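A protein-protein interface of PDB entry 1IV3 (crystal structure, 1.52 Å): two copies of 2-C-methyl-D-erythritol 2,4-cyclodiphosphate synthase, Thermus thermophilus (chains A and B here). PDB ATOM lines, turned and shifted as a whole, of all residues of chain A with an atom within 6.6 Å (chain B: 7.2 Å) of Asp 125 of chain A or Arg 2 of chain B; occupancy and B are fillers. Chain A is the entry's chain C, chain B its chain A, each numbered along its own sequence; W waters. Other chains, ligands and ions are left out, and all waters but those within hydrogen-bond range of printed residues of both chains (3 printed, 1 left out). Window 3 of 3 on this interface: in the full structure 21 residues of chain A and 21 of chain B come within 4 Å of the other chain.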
ATOM      1  N   LEU A  92      17.713   8.664   2.146  1.00  0.00           N
ATOM      2  CA  LEU A  92      18.135   9.722   1.233  1.00  0.00           C
ATOM      3  C   LEU A  92      17.041  10.193   0.300  1.00  0.00           C
ATOM      4  O   LEU A  92      17.046  11.325  -0.164  1.00  0.00           O
ATOM      5  CB  LEU A  92      19.344   9.207   0.430  1.00  0.00           C
ATOM      6  CG  LEU A  92      19.670  10.045  -0.812  1.00  0.00           C
ATOM      7  CD1 LEU A  92      20.572  11.212  -0.456  1.00  0.00           C
ATOM      8  CD2 LEU A  92      20.308   9.175  -1.888  1.00  0.00           C
ATOM      9  N   GLN A  93      16.065   9.345  -0.020  1.00  0.00           N
ATOM     10  CA  GLN A  93      15.119   9.672  -1.076  1.00  0.00           C
ATOM     11  C   GLN A  93      13.901   8.762  -1.063  1.00  0.00           C
ATOM     12  O   GLN A  93      14.017   7.570  -0.752  1.00  0.00           O
ATOM     13  CB  GLN A  93      15.812   9.528  -2.451  1.00  0.00           C
ATOM     14  CG  GLN A  93      14.967  10.146  -3.557  1.00  0.00           C
ATOM     15  CD  GLN A  93      15.714  10.495  -4.829  1.00  0.00           C
ATOM     16  OE1 GLN A  93      15.263  11.383  -5.580  1.00  0.00           O
ATOM     17  NE2 GLN A  93      16.826   9.818  -5.069  1.00  0.00           N
ATOM     18  N   VAL A 113       3.601  17.161  -1.010  1.00  0.00           N
ATOM     19  CA  VAL A 113       5.066  17.043  -0.964  1.00  0.00           C
ATOM     20  C   VAL A 113       5.612  17.608   0.340  1.00  0.00           C
ATOM     21  O   VAL A 113       6.480  17.008   0.990  1.00  0.00           O
ATOM     22  CB  VAL A 113       5.719  17.736  -2.185  1.00  0.00           C
ATOM     23  CG1 VAL A 113       7.220  17.851  -2.138  1.00  0.00           C
ATOM     24  CG2 VAL A 113       5.325  16.926  -3.435  1.00  0.00           C
ATOM     25  N   LEU A 122      13.156  14.836   4.690  1.00  0.00           N
ATOM     26  CA  LEU A 122      13.906  14.916   3.447  1.00  0.00           C
ATOM     27  C   LEU A 122      13.714  16.245   2.731  1.00  0.00           C
ATOM     28  O   LEU A 122      12.607  16.769   2.851  1.00  0.00           O
ATOM     29  CB  LEU A 122      13.448  13.827   2.456  1.00  0.00           C
ATOM     30  CG  LEU A 122      13.849  12.408   2.895  1.00  0.00           C
ATOM     31  CD1 LEU A 122      13.295  11.382   1.915  1.00  0.00           C
ATOM     32  CD2 LEU A 122      15.359  12.310   3.015  1.00  0.00           C
ATOM     33  N   PRO A 123      14.725  16.725   2.029  1.00  0.00           N
ATOM     34  CA  PRO A 123      14.569  17.986   1.293  1.00  0.00           C
ATOM     35  C   PRO A 123      13.576  17.774   0.159  1.00  0.00           C
ATOM     36  O   PRO A 123      13.455  16.649  -0.326  1.00  0.00           O
ATOM     37  CB  PRO A 123      15.965  18.298   0.753  1.00  0.00           C
ATOM     38  CG  PRO A 123      16.665  16.988   0.746  1.00  0.00           C
ATOM     39  CD  PRO A 123      16.081  16.169   1.864  1.00  0.00           C
ATOM     40  N   GLN A 124      12.892  18.829  -0.260  1.00  0.00           N
ATOM     41  CA  GLN A 124      11.810  18.666  -1.233  1.00  0.00           C
ATOM     42  C   GLN A 124      12.255  18.047  -2.549  1.00  0.00           C
ATOM     43  O   GLN A 124      11.440  17.393  -3.230  1.00  0.00           O
ATOM     44  CB  GLN A 124      11.165  20.037  -1.482  1.00  0.00           C
ATOM     45  CG  GLN A 124      10.586  20.640  -0.199  1.00  0.00           C
ATOM     46  CD  GLN A 124       9.111  20.960  -0.364  1.00  0.00           C
ATOM     47  OE1 GLN A 124       8.588  21.013  -1.481  1.00  0.00           O
ATOM     48  NE2 GLN A 124       8.421  21.195   0.746  1.00  0.00           N
ATOM     49  N   ASP A 125      13.515  18.257  -2.919  1.00  0.00           N
ATOM     50  CA  ASP A 125      13.977  17.685  -4.184  1.00  0.00           C
ATOM     51  C   ASP A 125      14.195  16.175  -4.058  1.00  0.00           C
ATOM     52  O   ASP A 125      14.513  15.551  -5.068  1.00  0.00           O
ATOM     53  CB  ASP A 125      15.264  18.381  -4.652  1.00  0.00           C
ATOM     54  CG  ASP A 125      16.401  18.132  -3.664  1.00  0.00           C
ATOM     55  OD1 ASP A 125      17.303  17.314  -3.957  1.00  0.00           O
ATOM     56  OD2 ASP A 125      16.359  18.749  -2.573  1.00  0.00           O
ATOM     57  N   ARG A 126      14.053  15.609  -2.862  1.00  0.00           N
ATOM     58  CA  ARG A 126      14.286  14.180  -2.630  1.00  0.00           C
ATOM     59  C   ARG A 126      12.987  13.451  -2.304  1.00  0.00           C
ATOM     60  O   ARG A 126      12.929  12.298  -1.872  1.00  0.00           O
ATOM     61  CB  ARG A 126      15.297  14.010  -1.486  1.00  0.00           C
ATOM     62  CG  ARG A 126      16.738  14.323  -1.849  1.00  0.00           C
ATOM     63  CD  ARG A 126      17.319  13.212  -2.713  1.00  0.00           C
ATOM     64  NE  ARG A 126      18.752  13.407  -2.934  1.00  0.00           N
ATOM     65  CZ  ARG A 126      19.562  12.462  -3.401  1.00  0.00           C
ATOM     66  NH1 ARG A 126      19.123  11.246  -3.702  1.00  0.00           N
ATOM     67  NH2 ARG A 126      20.848  12.755  -3.563  1.00  0.00           N
ATOM     68  N   ILE A 127      11.895  14.177  -2.501  1.00  0.00           N
ATOM     69  CA  ILE A 127      10.548  13.625  -2.460  1.00  0.00           C
ATOM     70  C   ILE A 127      10.050  13.630  -3.905  1.00  0.00           C
ATOM     71  O   ILE A 127       9.795  14.688  -4.506  1.00  0.00           O
ATOM     72  CB  ILE A 127       9.605  14.426  -1.556  1.00  0.00           C
ATOM     73  CG1 ILE A 127      10.029  14.506  -0.090  1.00  0.00           C
ATOM     74  CG2 ILE A 127       8.166  13.930  -1.713  1.00  0.00           C
ATOM     75  CD1 ILE A 127      10.021  13.244   0.742  1.00  0.00           C
ATOM     76  N   GLY A 128       9.973  12.437  -4.482  1.00  0.00           N
ATOM     77  CA  GLY A 128       9.513  12.355  -5.877  1.00  0.00           C
ATOM     78  C   GLY A 128       8.094  11.823  -5.917  1.00  0.00           C
ATOM     79  O   GLY A 128       7.893  10.601  -5.869  1.00  0.00           O
ATOM     80  N   LEU A 149      15.400   5.050  -1.020  1.00  0.00           N
ATOM     81  CA  LEU A 149      16.835   4.852  -1.159  1.00  0.00           C
ATOM     82  C   LEU A 149      17.514   5.265   0.133  1.00  0.00           C
ATOM     83  O   LEU A 149      17.162   6.339   0.636  1.00  0.00           O
ATOM     84  CB  LEU A 149      17.285   5.702  -2.350  1.00  0.00           C
ATOM     85  CG  LEU A 149      18.784   5.741  -2.643  1.00  0.00           C
ATOM     86  CD1 LEU A 149      19.283   4.341  -2.923  1.00  0.00           C
ATOM     87  CD2 LEU A 149      19.061   6.693  -3.803  1.00  0.00           C
ATOM     88  N   ARG B   2      20.762   9.164  -7.080  1.00  0.00           N
ATOM     89  CA  ARG B   2      19.325   9.433  -7.081  1.00  0.00           C
ATOM     90  C   ARG B   2      18.523   8.350  -7.785  1.00  0.00           C
ATOM     91  O   ARG B   2      19.010   7.701  -8.705  1.00  0.00           O
ATOM     92  CB  ARG B   2      19.004  10.743  -7.810  1.00  0.00           C
ATOM     93  CG  ARG B   2      19.469  11.955  -7.020  1.00  0.00           C
ATOM     94  CD  ARG B   2      18.998  13.250  -7.686  1.00  0.00           C
ATOM     95  NE  ARG B   2      19.339  14.351  -6.804  1.00  0.00           N
ATOM     96  CZ  ARG B   2      18.528  15.084  -6.076  1.00  0.00           C
ATOM     97  NH1 ARG B   2      17.233  14.852  -6.107  1.00  0.00           N
ATOM     98  NH2 ARG B   2      19.030  16.059  -5.319  1.00  0.00           N
ATOM     99  N   ILE B   3      17.284   8.207  -7.340  1.00  0.00           N
ATOM    100  CA  ILE B   3      16.433   7.194  -7.950  1.00  0.00           C
ATOM    101  C   ILE B   3      15.088   7.819  -8.303  1.00  0.00           C
ATOM    102  O   ILE B   3      14.689   8.771  -7.627  1.00  0.00           O
ATOM    103  CB  ILE B   3      16.206   5.966  -7.052  1.00  0.00           C
ATOM    104  CG1 ILE B   3      15.324   4.913  -7.732  1.00  0.00           C
ATOM    105  CG2 ILE B   3      15.605   6.331  -5.709  1.00  0.00           C
ATOM    106  CD1 ILE B   3      15.578   3.498  -7.301  1.00  0.00           C
ATOM    107  N   GLY B   4      14.446   7.284  -9.337  1.00  0.00           N
ATOM    108  CA  GLY B   4      13.116   7.820  -9.653  1.00  0.00           C
ATOM    109  C   GLY B   4      12.213   6.668 -10.088  1.00  0.00           C
ATOM    110  O   GLY B   4      12.706   5.736 -10.714  1.00  0.00           O
ATOM    111  N   LEU B  49      11.572  12.962 -13.786  1.00  0.00           N
ATOM    112  CA  LEU B  49      11.116  14.154 -13.061  1.00  0.00           C
ATOM    113  C   LEU B  49      11.117  13.877 -11.570  1.00  0.00           C
ATOM    114  O   LEU B  49      11.545  14.672 -10.731  1.00  0.00           O
ATOM    115  CB  LEU B  49       9.713  14.550 -13.522  1.00  0.00           C
ATOM    116  CG  LEU B  49       9.573  15.008 -14.981  1.00  0.00           C
ATOM    117  CD1 LEU B  49       8.110  15.322 -15.293  1.00  0.00           C
ATOM    118  CD2 LEU B  49      10.460  16.212 -15.254  1.00  0.00           C
ATOM    119  N   SER B  50      10.584  12.706 -11.234  1.00  0.00           N
ATOM    120  CA  SER B  50      10.478  12.259  -9.847  1.00  0.00           C
ATOM    121  C   SER B  50      11.833  12.245  -9.139  1.00  0.00           C
ATOM    122  O   SER B  50      11.918  12.583  -7.953  1.00  0.00           O
ATOM    123  CB  SER B  50       9.838  10.859  -9.823  1.00  0.00           C
ATOM    124  OG  SER B  50       9.342  10.615  -8.507  1.00  0.00           O
ATOM    125  N   ALA B  51      12.880  11.845  -9.856  1.00  0.00           N
ATOM    126  CA  ALA B  51      14.207  11.757  -9.260  1.00  0.00           C
ATOM    127  C   ALA B  51      14.695  13.108  -8.734  1.00  0.00           C
ATOM    128  O   ALA B  51      15.618  13.120  -7.919  1.00  0.00           O
ATOM    129  CB  ALA B  51      15.230  11.204 -10.240  1.00  0.00           C
ATOM    130  N   TYR B  52      14.105  14.206  -9.203  1.00  0.00           N
ATOM    131  CA  TYR B  52      14.473  15.526  -8.702  1.00  0.00           C
ATOM    132  C   TYR B  52      13.304  16.267  -8.099  1.00  0.00           C
ATOM    133  O   TYR B  52      13.410  17.461  -7.816  1.00  0.00           O
ATOM    134  CB  TYR B  52      15.105  16.354  -9.833  1.00  0.00           C
ATOM    135  CG  TYR B  52      16.578  16.047  -9.946  1.00  0.00           C
ATOM    136  CD1 TYR B  52      16.978  14.915 -10.654  1.00  0.00           C
ATOM    137  CD2 TYR B  52      17.530  16.856  -9.343  1.00  0.00           C
ATOM    138  CE1 TYR B  52      18.315  14.598 -10.769  1.00  0.00           C
ATOM    139  CE2 TYR B  52      18.872  16.543  -9.467  1.00  0.00           C
ATOM    140  CZ  TYR B  52      19.246  15.425 -10.178  1.00  0.00           C
ATOM    141  OH  TYR B  52      20.572  15.105 -10.307  1.00  0.00           O
ATOM    142  N   GLY B  53      12.181  15.586  -7.852  1.00  0.00           N
ATOM    143  CA  GLY B  53      11.058  16.245  -7.212  1.00  0.00           C
ATOM    144  C   GLY B  53      10.402  17.280  -8.114  1.00  0.00           C
ATOM    145  O   GLY B  53       9.725  18.170  -7.591  1.00  0.00           O
ATOM    146  N   LEU B  54      10.569  17.206  -9.430  1.00  0.00           N
ATOM    147  CA  LEU B  54      10.134  18.282 -10.318  1.00  0.00           C
ATOM    148  C   LEU B  54       8.663  18.264 -10.647  1.00  0.00           C
ATOM    149  O   LEU B  54       8.091  19.208 -11.185  1.00  0.00           O
ATOM    150  CB  LEU B  54      10.969  18.177 -11.601  1.00  0.00           C
ATOM    151  CG  LEU B  54      12.474  18.351 -11.319  1.00  0.00           C
ATOM    152  CD1 LEU B  54      13.269  18.023 -12.567  1.00  0.00           C
ATOM    153  CD2 LEU B  54      12.723  19.753 -10.801  1.00  0.00           C
ATOM    154  N   ARG B  87      20.355  20.287 -13.475  1.00  0.00           N
ATOM    155  CA  ARG B  87      20.505  20.242 -12.019  1.00  0.00           C
ATOM    156  C   ARG B  87      21.638  19.320 -11.596  1.00  0.00           C
ATOM    157  O   ARG B  87      21.717  18.990 -10.412  1.00  0.00           O
ATOM    158  CB  ARG B  87      19.161  19.850 -11.399  1.00  0.00           C
ATOM    159  CG  ARG B  87      18.162  21.018 -11.447  1.00  0.00           C
ATOM    160  CD  ARG B  87      16.736  20.492 -11.359  1.00  0.00           C
ATOM    161  NE  ARG B  87      15.714  21.521 -11.464  1.00  0.00           N
ATOM    162  CZ  ARG B  87      15.389  22.231 -12.535  1.00  0.00           C
ATOM    163  NH1 ARG B  87      15.994  22.079 -13.711  1.00  0.00           N
ATOM    164  NH2 ARG B  87      14.420  23.135 -12.429  1.00  0.00           N
ATOM    165  N   ALA B  89      22.377  16.194 -12.941  1.00  0.00           N
ATOM    166  CA  ALA B  89      22.235  14.738 -13.017  1.00  0.00           C
ATOM    167  C   ALA B  89      22.975  14.121 -14.187  1.00  0.00           C
ATOM    168  O   ALA B  89      23.122  14.715 -15.264  1.00  0.00           O
ATOM    169  CB  ALA B  89      20.746  14.447 -13.146  1.00  0.00           C
ATOM    170  N   VAL B 148      14.482   4.710 -12.651  1.00  0.00           N
ATOM    171  CA  VAL B 148      15.721   5.228 -13.252  1.00  0.00           C
ATOM    172  C   VAL B 148      16.732   5.456 -12.134  1.00  0.00           C
ATOM    173  O   VAL B 148      16.396   5.697 -10.956  1.00  0.00           O
ATOM    174  CB  VAL B 148      15.517   6.536 -14.039  1.00  0.00           C
ATOM    175  CG1 VAL B 148      14.631   6.325 -15.256  1.00  0.00           C
ATOM    176  CG2 VAL B 148      14.931   7.596 -13.120  1.00  0.00           C
ATOM    177  N   LEU B 149      17.998   5.368 -12.530  1.00  0.00           N
ATOM    178  CA  LEU B 149      19.083   5.581 -11.565  1.00  0.00           C
ATOM    179  C   LEU B 149      19.998   6.654 -12.140  1.00  0.00           C
ATOM    180  O   LEU B 149      20.317   6.570 -13.335  1.00  0.00           O
ATOM    181  CB  LEU B 149      19.794   4.260 -11.338  1.00  0.00           C
ATOM    182  CG  LEU B 149      20.942   4.202 -10.336  1.00  0.00           C
ATOM    183  CD1 LEU B 149      20.440   4.485  -8.931  1.00  0.00           C
ATOM    184  CD2 LEU B 149      21.638   2.843 -10.435  1.00  0.00           C
ATOM    185  N   LEU B 150      20.386   7.599 -11.310  1.00  0.00           N
ATOM    186  CA  LEU B 150      21.195   8.716 -11.786  1.00  0.00           C
ATOM    187  C   LEU B 150      22.362   9.007 -10.837  1.00  0.00           C
ATOM    188  O   LEU B 150      22.147   8.945  -9.629  1.00  0.00           O
ATOM    189  CB  LEU B 150      20.335   9.973 -11.911  1.00  0.00           C
ATOM    190  CG  LEU B 150      19.071   9.860 -12.769  1.00  0.00           C
ATOM    191  CD1 LEU B 150      17.858   9.748 -11.863  1.00  0.00           C
ATOM    192  CD2 LEU B 150      18.921  11.036 -13.712  1.00  0.00           C
ATOM    193  N   ASP B 151      23.498   9.323 -11.428  1.00  0.00           N
ATOM    194  CA  ASP B 151      24.775   9.658 -10.829  1.00  0.00           C
ATOM    195  C   ASP B 151      25.659   8.453 -10.554  1.00  0.00           C
ATOM    196  O   ASP B 151      26.750   8.248 -11.075  1.00  0.00           O
ATOM    197  CB  ASP B 151      24.531  10.405  -9.511  1.00  0.00           C
ATOM    198  CG  ASP B 151      24.064  11.819  -9.808  1.00  0.00           C
ATOM    199  OD1 ASP B 151      23.664  12.029 -10.980  1.00  0.00           O
ATOM    200  OD2 ASP B 151      24.119  12.649  -8.878  1.00  0.00           O
HETATM  201  O   HOH W   1       7.094   9.142  -8.659  1.00  0.00           O
HETATM  202  O   HOH W   2      19.937  15.785  -1.993  1.00  0.00           O
HETATM  203  O   HOH W   3       9.907  18.711  -4.861  1.00  0.00           O
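Arg 2 of chain B touches Gln 93 of chain A (CA to NE2, 3.2 Å).
O of Asp 125 of chain A touches O of Ala 51 of chain B, at 3.9 Å.
Tyr 52 of chain B touches Asp 125 of chain A (C to O, 3.3 Å).
Asp 125 of chain A touches Gly 53 of chain B.
NH1 of Arg 126 of chain A touches CG of Arg 2 of chain B, 3.4 Å away.
O of Ile 127 of chain A touches CA of Gly 53 of chain B, 3.4 Å away.
CG2 of Ile 3 of chain B touches CB of Leu 149 of chain A, at 3.8 Å.
Of chain B, only Arg 2, Ala 51, Tyr 52 and Gly 53 come within 4 Å of Asp 125 of chain A.
Arg 2 of chain B touches just these residues of chain A: Gln 93, Asp 125 and Arg 126.
Of the printed residues of chain A, Ile 3 of chain B touches Gln 93 (2.8 Å) and Leu 149 (3.8 Å).
Of the printed residues of chain B, Ile 127 of chain A touches Gly 53 (3.4 Å).
Gly 4 of chain B touches none of the printed residues of chain A.
Ala 89 of chain B touches none of the printed residues of chain A.
The nearest residue of chain B that does not touch Asp 125 of chain A is Ser 50 of chain B (4.9 Å).
The nearest residue of chain A that does not touch Arg 2 of chain B is Leu 149 of chain A (4.3 Å).
The nearest printed residue of chain B that does not touch Ile 127 of chain A is Ser 50 of chain B (4.6 Å).
The guanidinium group of Arg 2 of chain B lies within hydrogen-bond range of the backbone carbonyl oxygen of Ala 51 of chain B (3.0 Å).
The backbone carbonyl oxygen (O) of Leu 150 of chain B is in hydrogen-bond range of the backbone NH (N) of Arg 2 of chain B (2.9 Å).
OH of Tyr 52 of chain B lies close to N of Ala 89 of chain B (3.4 Å).
O of Leu 149 of chain A lies within hydrogen-bond range of N of Leu 92 of chain A, 2.8 Å away.
The side-chain amide nitrogen (NE2) of Gln 93 of chain A sits close to the guanidinium group (NH1) of Arg 126 of chain A (3.0 Å).
The backbone carbonyl oxygen (O) of Gln 93 of chain A lies within hydrogen-bond range of the backbone NH (N) of Leu 149 of chain A (2.9 Å).
The side-chain carboxylate (OD1) of Asp 125 of chain A is in salt-bridge range of the guanidinium group (NH2) of Arg 2 of chain B, 2.5 Å away.
NE2 of Gln 93 of chain A lies close to N of Ile 3 of chain B, at 2.8 Å.
The side-chain hydroxyl (OG) of Ser 50 of chain B is in hydrogen-bond range of the backbone carbonyl oxygen (O) of Gly 128 of chain A (3.0 Å).
OE1 of Gln 93 of chain A sits close to O of Ala 51 of chain B (2.9 Å).
Hydrophobic or aromatic side chains of chain A within 4 Å of the printed part of chain B: Leu 149.
Hydrophobic or aromatic side chains of chain B within 4 Å of the printed part of chain A: Ile 3.
Among the printed residues, 11 pairs touch across the chains.
1 position is printed for both chains.
Of the 11 pairs that touch across the chains among the printed residues, none has its exchanged pair printed and touching as well.
Water W3 lies within hydrogen-bond range of the backbone carbonyl oxygen (O) of Gln 124 of chain A and the backbone carbonyl oxygen (O) of Gly 53 of chain B.
Water W1 bridges OG of Ser 50 of chain B (2.7 Å) and O of Gly 128 of chain A (3.2 Å).
Water W2 lies within hydrogen-bond range of the guanidinium group (NE) of Arg 126 of chain A (2.8 Å) and the guanidinium group (NH2) of Arg 2 of chain B (3.5 Å).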
